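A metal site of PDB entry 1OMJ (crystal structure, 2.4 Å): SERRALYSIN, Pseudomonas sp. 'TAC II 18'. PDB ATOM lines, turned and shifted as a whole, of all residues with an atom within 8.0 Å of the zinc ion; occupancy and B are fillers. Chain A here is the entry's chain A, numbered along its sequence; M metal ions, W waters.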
ATOM      1  N   ALA A 130      -6.121  14.542  -1.101  1.00  0.00           N
ATOM      2  CA  ALA A 130      -5.964  13.688  -2.265  1.00  0.00           C
ATOM      3  C   ALA A 130      -4.548  13.097  -2.270  1.00  0.00           C
ATOM      4  O   ALA A 130      -3.651  13.646  -1.609  1.00  0.00           O
ATOM      5  CB  ALA A 130      -6.203  14.506  -3.560  1.00  0.00           C
ATOM      6  N   PHE A 131      -4.346  12.011  -3.009  1.00  0.00           N
ATOM      7  CA  PHE A 131      -3.029  11.375  -3.095  1.00  0.00           C
ATOM      8  C   PHE A 131      -2.892  10.461  -4.303  1.00  0.00           C
ATOM      9  O   PHE A 131      -3.888  10.055  -4.912  1.00  0.00           O
ATOM     10  CB  PHE A 131      -2.679  10.621  -1.802  1.00  0.00           C
ATOM     11  CG  PHE A 131      -3.657   9.543  -1.416  1.00  0.00           C
ATOM     12  CD1 PHE A 131      -3.451   8.217  -1.813  1.00  0.00           C
ATOM     13  CD2 PHE A 131      -4.754   9.831  -0.606  1.00  0.00           C
ATOM     14  CE1 PHE A 131      -4.318   7.205  -1.406  1.00  0.00           C
ATOM     15  CE2 PHE A 131      -5.650   8.829  -0.191  1.00  0.00           C
ATOM     16  CZ  PHE A 131      -5.432   7.514  -0.585  1.00  0.00           C
ATOM     17  N   ALA A 132      -1.647  10.141  -4.664  1.00  0.00           N
ATOM     18  CA  ALA A 132      -1.343   9.323  -5.829  1.00  0.00           C
ATOM     19  C   ALA A 132      -0.069   8.535  -5.574  1.00  0.00           C
ATOM     20  O   ALA A 132       0.658   8.833  -4.630  1.00  0.00           O
ATOM     21  CB  ALA A 132      -1.157  10.200  -7.035  1.00  0.00           C
ATOM     22  N   TYR A 162      -8.523  25.180  -7.636  1.00  0.00           N
ATOM     23  CA  TYR A 162      -7.650  24.154  -7.061  1.00  0.00           C
ATOM     24  C   TYR A 162      -8.156  22.742  -7.257  1.00  0.00           C
ATOM     25  O   TYR A 162      -7.386  21.781  -7.202  1.00  0.00           O
ATOM     26  CB  TYR A 162      -7.417  24.396  -5.581  1.00  0.00           C
ATOM     27  CG  TYR A 162      -6.196  23.658  -5.105  1.00  0.00           C
ATOM     28  CD1 TYR A 162      -6.294  22.633  -4.157  1.00  0.00           C
ATOM     29  CD2 TYR A 162      -4.943  23.973  -5.624  1.00  0.00           C
ATOM     30  CE1 TYR A 162      -5.156  21.946  -3.752  1.00  0.00           C
ATOM     31  CE2 TYR A 162      -3.805  23.282  -5.227  1.00  0.00           C
ATOM     32  CZ  TYR A 162      -3.920  22.282  -4.281  1.00  0.00           C
ATOM     33  OH  TYR A 162      -2.775  21.636  -3.865  1.00  0.00           O
ATOM     34  N   THR A 166      -5.573  20.065  -8.735  1.00  0.00           N
ATOM     35  CA  THR A 166      -5.343  18.878  -7.909  1.00  0.00           C
ATOM     36  C   THR A 166      -5.281  17.671  -8.842  1.00  0.00           C
ATOM     37  O   THR A 166      -4.377  16.851  -8.755  1.00  0.00           O
ATOM     38  CB  THR A 166      -6.464  18.684  -6.868  1.00  0.00           C
ATOM     39  OG1 THR A 166      -6.397  19.746  -5.907  1.00  0.00           O
ATOM     40  CG2 THR A 166      -6.308  17.351  -6.146  1.00  0.00           C
ATOM     41  N   HIS A 169      -2.134  17.817 -10.761  1.00  0.00           N
ATOM     42  CA  HIS A 169      -1.036  17.576  -9.811  1.00  0.00           C
ATOM     43  C   HIS A 169      -0.836  16.080  -9.499  1.00  0.00           C
ATOM     44  O   HIS A 169       0.297  15.560  -9.578  1.00  0.00           O
ATOM     45  CB  HIS A 169      -1.312  18.382  -8.525  1.00  0.00           C
ATOM     46  CG  HIS A 169      -0.321  18.171  -7.419  1.00  0.00           C
ATOM     47  ND1 HIS A 169       0.720  19.058  -7.172  1.00  0.00           N
ATOM     48  CD2 HIS A 169      -0.217  17.204  -6.478  1.00  0.00           C
ATOM     49  CE1 HIS A 169       1.413  18.625  -6.138  1.00  0.00           C
ATOM     50  NE2 HIS A 169       0.864  17.502  -5.696  1.00  0.00           N
ATOM     51  N   GLU A 170      -1.934  15.397  -9.138  1.00  0.00           N
ATOM     52  CA  GLU A 170      -1.925  13.969  -8.801  1.00  0.00           C
ATOM     53  C   GLU A 170      -1.556  13.109 -10.018  1.00  0.00           C
ATOM     54  O   GLU A 170      -0.876  12.089  -9.907  1.00  0.00           O
ATOM     55  CB  GLU A 170      -3.290  13.517  -8.284  1.00  0.00           C
ATOM     56  CG  GLU A 170      -3.749  14.124  -6.943  1.00  0.00           C
ATOM     57  CD  GLU A 170      -2.695  14.052  -5.845  1.00  0.00           C
ATOM     58  OE1 GLU A 170      -1.848  13.131  -5.879  1.00  0.00           O
ATOM     59  OE2 GLU A 170      -2.719  14.916  -4.921  1.00  0.00           O
ATOM     60  N   GLY A 172       0.293  14.152 -12.231  1.00  0.00           N
ATOM     61  CA  GLY A 172       1.720  14.408 -12.357  1.00  0.00           C
ATOM     62  C   GLY A 172       2.460  13.312 -11.622  1.00  0.00           C
ATOM     63  O   GLY A 172       3.350  12.669 -12.176  1.00  0.00           O
ATOM     64  N   HIS A 173       2.094  13.090 -10.356  1.00  0.00           N
ATOM     65  CA  HIS A 173       2.697  12.020  -9.554  1.00  0.00           C
ATOM     66  C   HIS A 173       2.615  10.665 -10.245  1.00  0.00           C
ATOM     67  O   HIS A 173       3.628   9.966 -10.357  1.00  0.00           O
ATOM     68  CB  HIS A 173       2.044  11.903  -8.171  1.00  0.00           C
ATOM     69  CG  HIS A 173       2.430  12.997  -7.213  1.00  0.00           C
ATOM     70  ND1 HIS A 173       3.737  13.387  -7.034  1.00  0.00           N
ATOM     71  CD2 HIS A 173       1.697  13.731  -6.354  1.00  0.00           C
ATOM     72  CE1 HIS A 173       3.795  14.322  -6.090  1.00  0.00           C
ATOM     73  NE2 HIS A 173       2.565  14.541  -5.659  1.00  0.00           N
ATOM     74  N   LEU A 177       6.436  12.326 -11.601  1.00  0.00           N
ATOM     75  CA  LEU A 177       6.988  13.580 -11.093  1.00  0.00           C
ATOM     76  C   LEU A 177       6.872  13.661  -9.577  1.00  0.00           C
ATOM     77  O   LEU A 177       5.891  13.205  -8.989  1.00  0.00           O
ATOM     78  CB  LEU A 177       6.306  14.792 -11.740  1.00  0.00           C
ATOM     79  CG  LEU A 177       6.381  14.897 -13.270  1.00  0.00           C
ATOM     80  CD1 LEU A 177       5.808  16.222 -13.725  1.00  0.00           C
ATOM     81  CD2 LEU A 177       7.799  14.784 -13.712  1.00  0.00           C
ATOM     82  N   SER A 178       7.912  14.212  -8.954  1.00  0.00           N
ATOM     83  CA  SER A 178       7.970  14.433  -7.514  1.00  0.00           C
ATOM     84  C   SER A 178       7.730  15.933  -7.229  1.00  0.00           C
ATOM     85  O   SER A 178       7.528  16.722  -8.136  1.00  0.00           O
ATOM     86  CB  SER A 178       9.351  14.070  -6.962  1.00  0.00           C
ATOM     87  OG  SER A 178       9.556  12.667  -6.904  1.00  0.00           O
ATOM     88  N   HIS A 179       7.761  16.304  -5.958  1.00  0.00           N
ATOM     89  CA  HIS A 179       7.626  17.696  -5.572  1.00  0.00           C
ATOM     90  C   HIS A 179       8.990  18.328  -5.776  1.00  0.00           C
ATOM     91  O   HIS A 179       9.983  17.627  -5.838  1.00  0.00           O
ATOM     92  CB  HIS A 179       7.292  17.808  -4.100  1.00  0.00           C
ATOM     93  CG  HIS A 179       5.947  17.293  -3.757  1.00  0.00           C
ATOM     94  ND1 HIS A 179       5.611  16.881  -2.486  1.00  0.00           N
ATOM     95  CD2 HIS A 179       4.822  17.169  -4.498  1.00  0.00           C
ATOM     96  CE1 HIS A 179       4.341  16.528  -2.458  1.00  0.00           C
ATOM     97  NE2 HIS A 179       3.838  16.691  -3.675  1.00  0.00           N
ATOM     98  N   PRO A 180       9.046  19.650  -5.881  1.00  0.00           N
ATOM     99  CA  PRO A 180      10.304  20.383  -6.064  1.00  0.00           C
ATOM    100  C   PRO A 180      11.307  20.112  -4.936  1.00  0.00           C
ATOM    101  O   PRO A 180      12.523  20.319  -5.082  1.00  0.00           O
ATOM    102  CB  PRO A 180       9.843  21.833  -6.091  1.00  0.00           C
ATOM    103  CG  PRO A 180       8.500  21.730  -6.776  1.00  0.00           C
ATOM    104  CD  PRO A 180       7.878  20.533  -6.108  1.00  0.00           C
ATOM    105  N   TYR A 183      10.636  18.789   1.374  1.00  0.00           N
ATOM    106  CA  TYR A 183       9.867  19.548   2.362  1.00  0.00           C
ATOM    107  C   TYR A 183       9.926  18.878   3.737  1.00  0.00           C
ATOM    108  O   TYR A 183      10.824  18.018   3.931  1.00  0.00           O
ATOM    109  CB  TYR A 183       8.388  19.680   1.911  1.00  0.00           C
ATOM    110  CG  TYR A 183       8.175  20.274   0.526  1.00  0.00           C
ATOM    111  CD1 TYR A 183       9.002  21.293   0.025  1.00  0.00           C
ATOM    112  CD2 TYR A 183       7.104  19.846  -0.273  1.00  0.00           C
ATOM    113  CE1 TYR A 183       8.775  21.863  -1.228  1.00  0.00           C
ATOM    114  CE2 TYR A 183       6.857  20.419  -1.526  1.00  0.00           C
ATOM    115  CZ  TYR A 183       7.693  21.430  -1.999  1.00  0.00           C
ATOM    116  OH  TYR A 183       7.440  22.025  -3.218  1.00  0.00           O
ATOM    117  N   VAL A 206       3.099  23.106 -11.181  1.00  0.00           N
ATOM    118  CA  VAL A 206       1.928  22.796 -10.381  1.00  0.00           C
ATOM    119  C   VAL A 206       2.240  21.740  -9.302  1.00  0.00           C
ATOM    120  O   VAL A 206       1.338  21.337  -8.567  1.00  0.00           O
ATOM    121  CB  VAL A 206       0.759  22.257 -11.233  1.00  0.00           C
ATOM    122  CG1 VAL A 206       0.395  23.243 -12.324  1.00  0.00           C
ATOM    123  CG2 VAL A 206       1.121  20.899 -11.813  1.00  0.00           C
ATOM    124  N   MET A 207       3.485  21.284  -9.208  1.00  0.00           N
ATOM    125  CA  MET A 207       3.804  20.272  -8.191  1.00  0.00           C
ATOM    126  C   MET A 207       4.226  20.948  -6.882  1.00  0.00           C
ATOM    127  O   MET A 207       4.299  20.302  -5.850  1.00  0.00           O
ATOM    128  CB  MET A 207       4.929  19.323  -8.644  1.00  0.00           C
ATOM    129  CG  MET A 207       4.666  18.564  -9.953  1.00  0.00           C
ATOM    130  SD  MET A 207       3.154  17.576  -9.944  1.00  0.00           S
ATOM    131  CE  MET A 207       3.461  16.483  -8.480  1.00  0.00           C
ATOM    132  N   SER A 208       4.491  22.244  -6.956  1.00  0.00           N
ATOM    133  CA  SER A 208       4.926  23.001  -5.802  1.00  0.00           C
ATOM    134  C   SER A 208       3.830  23.166  -4.767  1.00  0.00           C
ATOM    135  O   SER A 208       2.637  23.114  -5.078  1.00  0.00           O
ATOM    136  CB  SER A 208       5.407  24.398  -6.237  1.00  0.00           C
ATOM    137  OG  SER A 208       5.815  25.176  -5.093  1.00  0.00           O
ATOM    138  N   TYR A 209       4.239  23.366  -3.524  1.00  0.00           N
ATOM    139  CA  TYR A 209       3.316  23.601  -2.407  1.00  0.00           C
ATOM    140  C   TYR A 209       3.209  25.106  -2.138  1.00  0.00           C
ATOM    141  O   TYR A 209       2.310  25.557  -1.456  1.00  0.00           O
ATOM    142  CB  TYR A 209       3.851  22.929  -1.146  1.00  0.00           C
ATOM    143  CG  TYR A 209       3.454  21.495  -0.942  1.00  0.00           C
ATOM    144  CD1 TYR A 209       3.062  20.689  -2.013  1.00  0.00           C
ATOM    145  CD2 TYR A 209       3.489  20.924   0.318  1.00  0.00           C
ATOM    146  CE1 TYR A 209       2.691  19.355  -1.813  1.00  0.00           C
ATOM    147  CE2 TYR A 209       3.128  19.594   0.526  1.00  0.00           C
ATOM    148  CZ  TYR A 209       2.741  18.815  -0.537  1.00  0.00           C
ATOM    149  OH  TYR A 209       2.374  17.507  -0.295  1.00  0.00           O
HETATM  150 ZN    ZN M   1       1.851  16.169  -4.318  1.00  0.00          ZN
HETATM  151  O   HOH W   1      -0.086  15.413  -2.993  1.00  0.00           O
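NE2 of His 179 binds the zinc ion (2.2 Å). A ring nitrogen (NE2) of His 169 binds the zinc ion. NE2 of His 173 is bound to the zinc ion, at 2.2 Å. The zinc ion is bound by water W1 (2.5 Å). The zinc ion has four donor atoms within binding distance.
A ring nitrogen (ND1) of His 169 sits at hydrogen-bond distance from the backbone carbonyl oxygen (O) of Val 206 (2.7 Å). O of Leu 177 is in hydrogen-bond range of ND1 of His 173, 2.9 Å away.
Within 4 Å of the zinc ion: His 169, His 173 and His 179. The nearest printed residue that does not touch the zinc ion is Tyr 209 (4.1 Å).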
